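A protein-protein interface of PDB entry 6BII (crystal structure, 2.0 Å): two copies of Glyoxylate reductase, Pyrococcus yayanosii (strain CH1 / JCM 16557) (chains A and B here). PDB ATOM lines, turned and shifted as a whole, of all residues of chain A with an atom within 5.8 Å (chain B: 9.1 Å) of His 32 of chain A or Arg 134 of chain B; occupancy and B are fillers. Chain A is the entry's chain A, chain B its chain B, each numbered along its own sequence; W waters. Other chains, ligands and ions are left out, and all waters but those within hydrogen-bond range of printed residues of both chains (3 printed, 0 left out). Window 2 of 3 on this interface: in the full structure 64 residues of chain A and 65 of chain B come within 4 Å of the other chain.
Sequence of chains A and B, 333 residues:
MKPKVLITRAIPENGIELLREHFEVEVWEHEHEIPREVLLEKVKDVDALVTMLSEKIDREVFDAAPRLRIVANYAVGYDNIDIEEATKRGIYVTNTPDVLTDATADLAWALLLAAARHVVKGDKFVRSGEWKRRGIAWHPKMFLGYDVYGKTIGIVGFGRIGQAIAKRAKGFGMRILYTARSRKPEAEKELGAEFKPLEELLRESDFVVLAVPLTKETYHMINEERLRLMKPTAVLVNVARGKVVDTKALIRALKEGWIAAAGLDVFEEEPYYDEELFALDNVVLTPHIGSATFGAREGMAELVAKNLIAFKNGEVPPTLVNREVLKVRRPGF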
ATOM      1  N   ARG A   9      30.656 -18.034   3.066  1.00  0.00           N
ATOM      2  CA  ARG A   9      30.324 -16.730   2.467  1.00  0.00           C
ATOM      3  C   ARG A   9      31.317 -15.676   2.901  1.00  0.00           C
ATOM      4  O   ARG A   9      31.977 -15.822   3.942  1.00  0.00           O
ATOM      5  CB  ARG A   9      28.926 -16.274   2.893  1.00  0.00           C
ATOM      6  CG  ARG A   9      28.142 -15.607   1.780  1.00  0.00           C
ATOM      7  CD  ARG A   9      27.547 -16.647   0.872  1.00  0.00           C
ATOM      8  NE  ARG A   9      26.525 -16.128  -0.003  1.00  0.00           N
ATOM      9  CZ  ARG A   9      26.750 -15.650  -1.208  1.00  0.00           C
ATOM     10  NH1 ARG A   9      27.973 -15.599  -1.720  1.00  0.00           N
ATOM     11  NH2 ARG A   9      25.723 -15.242  -1.937  1.00  0.00           N
ATOM     12  N   TRP A  28      34.630 -19.207   1.215  1.00  0.00           N
ATOM     13  CA  TRP A  28      33.993 -19.209  -0.094  1.00  0.00           C
ATOM     14  C   TRP A  28      33.731 -17.748  -0.466  1.00  0.00           C
ATOM     15  O   TRP A  28      32.858 -17.081   0.091  1.00  0.00           O
ATOM     16  CB  TRP A  28      32.693 -20.008  -0.060  1.00  0.00           C
ATOM     17  CG  TRP A  28      31.953 -19.985  -1.343  1.00  0.00           C
ATOM     18  CD1 TRP A  28      30.868 -19.202  -1.657  1.00  0.00           C
ATOM     19  CD2 TRP A  28      32.244 -20.761  -2.516  1.00  0.00           C
ATOM     20  NE1 TRP A  28      30.482 -19.441  -2.948  1.00  0.00           N
ATOM     21  CE2 TRP A  28      31.308 -20.392  -3.501  1.00  0.00           C
ATOM     22  CE3 TRP A  28      33.217 -21.697  -2.836  1.00  0.00           C
ATOM     23  CZ2 TRP A  28      31.274 -20.982  -4.766  1.00  0.00           C
ATOM     24  CZ3 TRP A  28      33.191 -22.289  -4.091  1.00  0.00           C
ATOM     25  CH2 TRP A  28      32.235 -21.914  -5.049  1.00  0.00           C
ATOM     26  N   HIS A  30      33.035 -16.247  -3.490  1.00  0.00           N
ATOM     27  CA  HIS A  30      32.303 -15.929  -4.714  1.00  0.00           C
ATOM     28  C   HIS A  30      30.941 -15.235  -4.452  1.00  0.00           C
ATOM     29  O   HIS A  30      30.372 -15.339  -3.361  1.00  0.00           O
ATOM     30  CB  HIS A  30      32.094 -17.230  -5.492  1.00  0.00           C
ATOM     31  CG  HIS A  30      33.365 -17.902  -5.911  1.00  0.00           C
ATOM     32  ND1 HIS A  30      34.067 -17.534  -7.034  1.00  0.00           N
ATOM     33  CD2 HIS A  30      34.037 -18.950  -5.382  1.00  0.00           C
ATOM     34  CE1 HIS A  30      35.120 -18.317  -7.169  1.00  0.00           C
ATOM     35  NE2 HIS A  30      35.112 -19.201  -6.191  1.00  0.00           N
ATOM     36  N   GLU A  31      30.439 -14.528  -5.444  1.00  0.00           N
ATOM     37  CA  GLU A  31      29.159 -13.854  -5.323  1.00  0.00           C
ATOM     38  C   GLU A  31      28.032 -14.859  -5.169  1.00  0.00           C
ATOM     39  O   GLU A  31      27.220 -14.733  -4.254  1.00  0.00           O
ATOM     40  CB  GLU A  31      28.923 -12.904  -6.510  1.00  0.00           C
ATOM     41  CG  GLU A  31      29.403 -11.469  -6.241  1.00  0.00           C
ATOM     42  CD  GLU A  31      28.249 -10.475  -6.150  1.00  0.00           C
ATOM     43  OE1 GLU A  31      28.037  -9.862  -5.068  1.00  0.00           O
ATOM     44  OE2 GLU A  31      27.544 -10.354  -7.179  1.00  0.00           O
ATOM     45  N   HIS A  32      28.017 -15.868  -6.034  1.00  0.00           N
ATOM     46  CA  HIS A  32      27.019 -16.948  -5.917  1.00  0.00           C
ATOM     47  C   HIS A  32      27.238 -17.796  -4.666  1.00  0.00           C
ATOM     48  O   HIS A  32      28.351 -17.928  -4.182  1.00  0.00           O
ATOM     49  CB  HIS A  32      26.946 -17.810  -7.175  1.00  0.00           C
ATOM     50  CG  HIS A  32      26.218 -17.154  -8.321  1.00  0.00           C
ATOM     51  ND1 HIS A  32      26.813 -16.224  -9.157  1.00  0.00           N
ATOM     52  CD2 HIS A  32      24.948 -17.312  -8.782  1.00  0.00           C
ATOM     53  CE1 HIS A  32      25.942 -15.836 -10.072  1.00  0.00           C
ATOM     54  NE2 HIS A  32      24.806 -16.486  -9.871  1.00  0.00           N
ATOM     55  N   GLU A  33      26.138 -18.329  -4.137  1.00  0.00           N
ATOM     56  CA  GLU A  33      26.170 -19.253  -3.006  1.00  0.00           C
ATOM     57  C   GLU A  33      26.967 -20.496  -3.397  1.00  0.00           C
ATOM     58  O   GLU A  33      27.089 -20.842  -4.559  1.00  0.00           O
ATOM     59  CB  GLU A  33      24.753 -19.662  -2.584  1.00  0.00           C
ATOM     60  CG  GLU A  33      24.095 -18.684  -1.602  1.00  0.00           C
ATOM     61  CD  GLU A  33      23.069 -17.717  -2.160  1.00  0.00           C
ATOM     62  OE1 GLU A  33      22.635 -17.779  -3.339  1.00  0.00           O
ATOM     63  OE2 GLU A  33      22.584 -16.893  -1.342  1.00  0.00           O
ATOM     64  N   ILE A  34      27.538 -21.128  -2.391  1.00  0.00           N
ATOM     65  CA  ILE A  34      28.351 -22.319  -2.613  1.00  0.00           C
ATOM     66  C   ILE A  34      27.458 -23.431  -3.194  1.00  0.00           C
ATOM     67  O   ILE A  34      26.403 -23.712  -2.633  1.00  0.00           O
ATOM     68  CB  ILE A  34      29.083 -22.761  -1.328  1.00  0.00           C
ATOM     69  CG1 ILE A  34      30.141 -23.817  -1.670  1.00  0.00           C
ATOM     70  CG2 ILE A  34      28.112 -23.274  -0.263  1.00  0.00           C
ATOM     71  CD1 ILE A  34      31.085 -24.091  -0.521  1.00  0.00           C
ATOM     72  N   PHE B 125      14.319  -4.050  -7.066  1.00  0.00           N
ATOM     73  CA  PHE B 125      15.236  -5.197  -7.232  1.00  0.00           C
ATOM     74  C   PHE B 125      14.454  -6.526  -7.243  1.00  0.00           C
ATOM     75  O   PHE B 125      14.707  -7.397  -8.091  1.00  0.00           O
ATOM     76  CB  PHE B 125      16.272  -5.167  -6.133  1.00  0.00           C
ATOM     77  CG  PHE B 125      17.353  -6.198  -6.261  1.00  0.00           C
ATOM     78  CD1 PHE B 125      18.355  -6.053  -7.205  1.00  0.00           C
ATOM     79  CD2 PHE B 125      17.425  -7.257  -5.368  1.00  0.00           C
ATOM     80  CE1 PHE B 125      19.378  -6.966  -7.307  1.00  0.00           C
ATOM     81  CE2 PHE B 125      18.457  -8.179  -5.467  1.00  0.00           C
ATOM     82  CZ  PHE B 125      19.440  -8.031  -6.436  1.00  0.00           C
ATOM     83  N   SER B 128      11.202  -6.324 -10.278  1.00  0.00           N
ATOM     84  CA  SER B 128      11.674  -6.353 -11.675  1.00  0.00           C
ATOM     85  C   SER B 128      12.183  -7.713 -12.094  1.00  0.00           C
ATOM     86  O   SER B 128      12.468  -7.916 -13.286  1.00  0.00           O
ATOM     87  CB  SER B 128      12.842  -5.380 -11.843  1.00  0.00           C
ATOM     88  OG  SER B 128      14.006  -5.789 -11.081  1.00  0.00           O
ATOM     89  N   GLY B 129      12.376  -8.620 -11.130  1.00  0.00           N
ATOM     90  CA  GLY B 129      13.000  -9.893 -11.411  1.00  0.00           C
ATOM     91  C   GLY B 129      14.520  -9.864 -11.398  1.00  0.00           C
ATOM     92  O   GLY B 129      15.138 -10.893 -11.658  1.00  0.00           O
ATOM     93  N   GLU B 130      15.129  -8.726 -11.059  1.00  0.00           N
ATOM     94  CA  GLU B 130      16.599  -8.665 -10.988  1.00  0.00           C
ATOM     95  C   GLU B 130      17.152  -9.663  -9.939  1.00  0.00           C
ATOM     96  O   GLU B 130      18.089 -10.423 -10.215  1.00  0.00           O
ATOM     97  CB  GLU B 130      17.094  -7.239 -10.742  1.00  0.00           C
ATOM     98  CG  GLU B 130      18.602  -7.099 -10.981  1.00  0.00           C
ATOM     99  CD  GLU B 130      19.171  -5.739 -10.655  1.00  0.00           C
ATOM    100  OE1 GLU B 130      18.458  -4.725 -10.532  1.00  0.00           O
ATOM    101  OE2 GLU B 130      20.389  -5.689 -10.508  1.00  0.00           O
ATOM    102  N   TRP B 131      16.518  -9.705  -8.774  1.00  0.00           N
ATOM    103  CA  TRP B 131      16.925 -10.642  -7.713  1.00  0.00           C
ATOM    104  C   TRP B 131      16.961 -12.060  -8.234  1.00  0.00           C
ATOM    105  O   TRP B 131      17.950 -12.770  -8.122  1.00  0.00           O
ATOM    106  CB  TRP B 131      15.949 -10.530  -6.546  1.00  0.00           C
ATOM    107  CG  TRP B 131      16.352 -11.216  -5.278  1.00  0.00           C
ATOM    108  CD1 TRP B 131      17.618 -11.497  -4.855  1.00  0.00           C
ATOM    109  CD2 TRP B 131      15.481 -11.606  -4.212  1.00  0.00           C
ATOM    110  NE1 TRP B 131      17.586 -12.077  -3.619  1.00  0.00           N
ATOM    111  CE2 TRP B 131      16.291 -12.136  -3.184  1.00  0.00           C
ATOM    112  CE3 TRP B 131      14.087 -11.585  -4.037  1.00  0.00           C
ATOM    113  CZ2 TRP B 131      15.756 -12.627  -1.972  1.00  0.00           C
ATOM    114  CZ3 TRP B 131      13.557 -12.051  -2.844  1.00  0.00           C
ATOM    115  CH2 TRP B 131      14.392 -12.566  -1.827  1.00  0.00           C
ATOM    116  N   LYS B 132      15.870 -12.455  -8.876  1.00  0.00           N
ATOM    117  CA  LYS B 132      15.768 -13.779  -9.438  1.00  0.00           C
ATOM    118  C   LYS B 132      16.769 -14.013 -10.552  1.00  0.00           C
ATOM    119  O   LYS B 132      17.403 -15.051 -10.616  1.00  0.00           O
ATOM    120  CB  LYS B 132      14.332 -13.985  -9.980  1.00  0.00           C
ATOM    121  CG  LYS B 132      14.044 -15.313 -10.671  1.00  0.00           C
ATOM    122  CD  LYS B 132      14.138 -16.455  -9.685  1.00  0.00           C
ATOM    123  CE  LYS B 132      13.511 -17.732 -10.226  1.00  0.00           C
ATOM    124  NZ  LYS B 132      14.064 -18.863  -9.453  1.00  0.00           N
ATOM    125  N   ARG B 133      16.885 -13.063 -11.460  1.00  0.00           N
ATOM    126  CA  ARG B 133      17.764 -13.210 -12.638  1.00  0.00           C
ATOM    127  C   ARG B 133      19.209 -13.398 -12.175  1.00  0.00           C
ATOM    128  O   ARG B 133      19.890 -14.255 -12.704  1.00  0.00           O
ATOM    129  CB  ARG B 133      17.640 -11.933 -13.504  1.00  0.00           C
ATOM    130  CG  ARG B 133      17.856 -11.915 -14.978  1.00  0.00           C
ATOM    131  CD  ARG B 133      16.813 -10.960 -15.637  1.00  0.00           C
ATOM    132  NE  ARG B 133      16.819  -9.548 -15.205  1.00  0.00           N
ATOM    133  CZ  ARG B 133      15.756  -8.836 -14.782  1.00  0.00           C
ATOM    134  NH1 ARG B 133      14.520  -9.364 -14.646  1.00  0.00           N
ATOM    135  NH2 ARG B 133      15.938  -7.563 -14.441  1.00  0.00           N
ATOM    136  N   ARG B 134      19.652 -12.636 -11.162  1.00  0.00           N
ATOM    137  CA  ARG B 134      21.015 -12.801 -10.643  1.00  0.00           C
ATOM    138  C   ARG B 134      21.270 -14.124  -9.938  1.00  0.00           C
ATOM    139  O   ARG B 134      22.419 -14.559  -9.865  1.00  0.00           O
ATOM    140  CB  ARG B 134      21.395 -11.646  -9.763  1.00  0.00           C
ATOM    141  CG  ARG B 134      21.555 -10.365 -10.532  1.00  0.00           C
ATOM    142  CD  ARG B 134      21.725  -9.229  -9.544  1.00  0.00           C
ATOM    143  NE  ARG B 134      22.114  -7.994 -10.214  1.00  0.00           N
ATOM    144  CZ  ARG B 134      23.359  -7.685 -10.572  1.00  0.00           C
ATOM    145  NH1 ARG B 134      24.367  -8.527 -10.344  1.00  0.00           N
ATOM    146  NH2 ARG B 134      23.606  -6.525 -11.176  1.00  0.00           N
ATOM    147  N   GLY B 135      20.222 -14.776  -9.435  1.00  0.00           N
ATOM    148  CA  GLY B 135      20.377 -16.110  -8.892  1.00  0.00           C
ATOM    149  C   GLY B 135      20.975 -16.197  -7.476  1.00  0.00           C
ATOM    150  O   GLY B 135      21.298 -17.279  -7.022  1.00  0.00           O
ATOM    151  N   ILE B 136      21.116 -15.069  -6.790  1.00  0.00           N
ATOM    152  CA  ILE B 136      21.728 -15.041  -5.467  1.00  0.00           C
ATOM    153  C   ILE B 136      20.649 -14.704  -4.447  1.00  0.00           C
ATOM    154  O   ILE B 136      20.062 -13.616  -4.471  1.00  0.00           O
ATOM    155  CB  ILE B 136      22.850 -13.993  -5.431  1.00  0.00           C
ATOM    156  CG1 ILE B 136      23.911 -14.348  -6.463  1.00  0.00           C
ATOM    157  CG2 ILE B 136      23.491 -13.901  -4.044  1.00  0.00           C
ATOM    158  CD1 ILE B 136      24.905 -13.234  -6.684  1.00  0.00           C
ATOM    159  N   ALA B 137      20.437 -15.616  -3.509  1.00  0.00           N
ATOM    160  CA  ALA B 137      19.409 -15.432  -2.485  1.00  0.00           C
ATOM    161  C   ALA B 137      19.737 -14.313  -1.499  1.00  0.00           C
ATOM    162  O   ALA B 137      18.938 -13.393  -1.229  1.00  0.00           O
ATOM    163  CB  ALA B 137      19.208 -16.754  -1.748  1.00  0.00           C
ATOM    164  N   TRP B 138      20.950 -14.389  -0.976  1.00  0.00           N
ATOM    165  CA  TRP B 138      21.324 -13.612   0.223  1.00  0.00           C
ATOM    166  C   TRP B 138      22.831 -13.422   0.196  1.00  0.00           C
ATOM    167  O   TRP B 138      23.559 -14.297  -0.259  1.00  0.00           O
ATOM    168  CB  TRP B 138      20.910 -14.365   1.493  1.00  0.00           C
ATOM    169  CG  TRP B 138      21.004 -13.619   2.778  1.00  0.00           C
ATOM    170  CD1 TRP B 138      20.013 -12.895   3.391  1.00  0.00           C
ATOM    171  CD2 TRP B 138      22.133 -13.562   3.650  1.00  0.00           C
ATOM    172  NE1 TRP B 138      20.460 -12.385   4.599  1.00  0.00           N
ATOM    173  CE2 TRP B 138      21.749 -12.795   4.789  1.00  0.00           C
ATOM    174  CE3 TRP B 138      23.420 -14.110   3.600  1.00  0.00           C
ATOM    175  CZ2 TRP B 138      22.604 -12.548   5.839  1.00  0.00           C
ATOM    176  CZ3 TRP B 138      24.279 -13.867   4.658  1.00  0.00           C
ATOM    177  CH2 TRP B 138      23.861 -13.095   5.762  1.00  0.00           C
ATOM    178  N   HIS B 139      23.292 -12.263   0.642  1.00  0.00           N
ATOM    179  CA  HIS B 139      24.728 -11.987   0.655  1.00  0.00           C
ATOM    180  C   HIS B 139      24.978 -11.037   1.825  1.00  0.00           C
ATOM    181  O   HIS B 139      24.189 -10.101   2.052  1.00  0.00           O
ATOM    182  CB  HIS B 139      25.248 -11.395  -0.679  1.00  0.00           C
ATOM    183  CG  HIS B 139      26.750 -11.334  -0.773  1.00  0.00           C
ATOM    184  ND1 HIS B 139      27.513 -10.431  -0.063  1.00  0.00           N
ATOM    185  CD2 HIS B 139      27.629 -12.084  -1.485  1.00  0.00           C
ATOM    186  CE1 HIS B 139      28.798 -10.640  -0.318  1.00  0.00           C
ATOM    187  NE2 HIS B 139      28.896 -11.628  -1.188  1.00  0.00           N
ATOM    188  N   PRO B 140      26.050 -11.277   2.581  1.00  0.00           N
ATOM    189  CA  PRO B 140      26.348 -10.419   3.742  1.00  0.00           C
ATOM    190  C   PRO B 140      26.534  -8.921   3.436  1.00  0.00           C
ATOM    191  O   PRO B 140      26.375  -8.117   4.348  1.00  0.00           O
ATOM    192  CB  PRO B 140      27.659 -11.007   4.289  1.00  0.00           C
ATOM    193  CG  PRO B 140      27.708 -12.410   3.797  1.00  0.00           C
ATOM    194  CD  PRO B 140      26.976 -12.422   2.479  1.00  0.00           C
ATOM    195  N   MET B 142      24.825  -7.340   0.717  1.00  0.00           N
ATOM    196  CA  MET B 142      23.726  -6.896  -0.151  1.00  0.00           C
ATOM    197  C   MET B 142      22.883  -5.825   0.569  1.00  0.00           C
ATOM    198  O   MET B 142      22.321  -6.086   1.646  1.00  0.00           O
ATOM    199  CB  MET B 142      22.850  -8.120  -0.545  1.00  0.00           C
ATOM    200  CG  MET B 142      21.650  -7.851  -1.439  1.00  0.00           C
ATOM    201  SD  MET B 142      20.590  -9.266  -1.942  1.00  0.00           S
ATOM    202  CE  MET B 142      21.734 -10.267  -2.880  1.00  0.00           C
ATOM    203  N   PHE B 143      22.760  -4.649  -0.049  1.00  0.00           N
ATOM    204  CA  PHE B 143      21.785  -3.614   0.373  1.00  0.00           C
ATOM    205  C   PHE B 143      22.011  -3.117   1.818  1.00  0.00           C
ATOM    206  O   PHE B 143      21.064  -2.807   2.562  1.00  0.00           O
ATOM    207  CB  PHE B 143      20.320  -4.092   0.166  1.00  0.00           C
ATOM    208  CG  PHE B 143      19.814  -3.925  -1.243  1.00  0.00           C
ATOM    209  CD1 PHE B 143      19.440  -2.694  -1.697  1.00  0.00           C
ATOM    210  CD2 PHE B 143      19.740  -4.990  -2.102  1.00  0.00           C
ATOM    211  CE1 PHE B 143      19.019  -2.517  -2.989  1.00  0.00           C
ATOM    212  CE2 PHE B 143      19.309  -4.833  -3.412  1.00  0.00           C
ATOM    213  CZ  PHE B 143      18.930  -3.584  -3.848  1.00  0.00           C
HETATM  214  O   HOH W   1      23.776 -18.369  -5.827  1.00  0.00           O
HETATM  215  O   HOH W   2      31.310 -12.252  -2.357  1.00  0.00           O
HETATM  216  O   HOH W   3      24.073 -16.848   1.191  1.00  0.00           O
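Of the printed residues of chain B, His 32 of chain A touches Arg 134 (3.1 Å) and Ile 136 (3.9 Å). Printed residues of chain A within 4 Å of Arg 134 of chain B: His 32. Printed residues of chain A within 4 Å of Gly 135 of chain B: Glu 33 (3.9 Å). Of the printed residues of chain B, Glu 33 of chain A touches Gly 135 (3.9 Å), Ile 136 (3.6 Å), Ala 137 (3.1 Å) and Trp 138 (3.0 Å). Printed residues of chain A within 4 Å of Trp 138 of chain B: Arg 9 and Glu 33. Of the printed residues of chain A, His 139 of chain B touches Arg 9 and Glu 31. Printed residues of chain B within 4 Å of Glu 31 of chain A: Ile 136 and His 139. The nearest residue of chain B that does not touch His 32 of chain A is Gly 135 of chain B (4.1 Å). The nearest residue of chain A that does not touch Arg 134 of chain B is Glu 31 of chain A (4.8 Å).
NH1 of Arg 9 of chain A lies within hydrogen-bond range of O of Glu 31 of chain A, at 2.8 Å. O of His 32 of chain A is in hydrogen-bond range of NH1 of Arg 9 of chain A. OE2 of Glu 33 of chain A is in salt-bridge range of NH2 of Arg 9 of chain A (3.6 Å). The side-chain carboxylate of Glu 130 of chain B lies within salt-bridge range of the guanidinium group of Arg 134 of chain B, at 2.9 Å. The indole nitrogen (NE1) of Trp 131 of chain B is in hydrogen-bond range of the backbone carbonyl oxygen (O) of Ile 136 of chain B (3.0 Å). O of Ala 137 of chain B is in hydrogen-bond range of NE1 of Trp 131 of chain B (3.0 Å).
Of the 16 printed residues of chain B, 7 touch a printed residue of chain A.
The backbone carbonyl oxygen (O) of Trp 138 of chain B is in hydrogen-bond range of the guanidinium group (NH2) of Arg 9 of chain A (2.9 Å). The backbone carbonyl oxygen (O) of Arg 134 of chain B lies within hydrogen-bond range of a ring nitrogen (NE2) of His 32 of chain A (3.1 Å). The side-chain carboxylate of Glu 33 of chain A lies within hydrogen-bond range of the backbone NH of Ala 137 of chain B, 3.1 Å away. The side-chain carboxylate (OE2) of Glu 33 of chain A is in hydrogen-bond range of the backbone NH (N) of Trp 138 of chain B, at 3.0 Å.
Ile 136 of chain B touches Arg 9 of chain A. Arg 9 of chain A touches His 139 of chain B. CD of Pro 140 of chain B touches CG of Arg 9 of chain A (3.5 Å). O of Glu 31 of chain A touches CD1 of Ile 136 of chain B, at 3.7 Å. Glu 31 of chain A touches His 139 of chain B. CD2 of His 32 of chain A touches CG1 of Ile 136 of chain B, 3.9 Å away. Gly 135 of chain B touches Glu 33 of chain A. Glu 33 of chain A touches Ile 136 of chain B.
Water W2 lies within hydrogen-bond range of a ring nitrogen (NE2) of His 139 of chain B (2.8 Å) and the backbone carbonyl oxygen of His 30 of chain A (3.4 Å). Water W1 lies within hydrogen-bond range of the side-chain carboxylate of Glu 33 of chain A and the backbone carbonyl oxygen of Gly 135 of chain B. Water W3 lies within hydrogen-bond range of the guanidinium group of Arg 9 of chain A, the side-chain carboxylate of Glu 33 of chain A and the backbone carbonyl oxygen of Trp 138 of chain B.
No position is printed for both chains.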
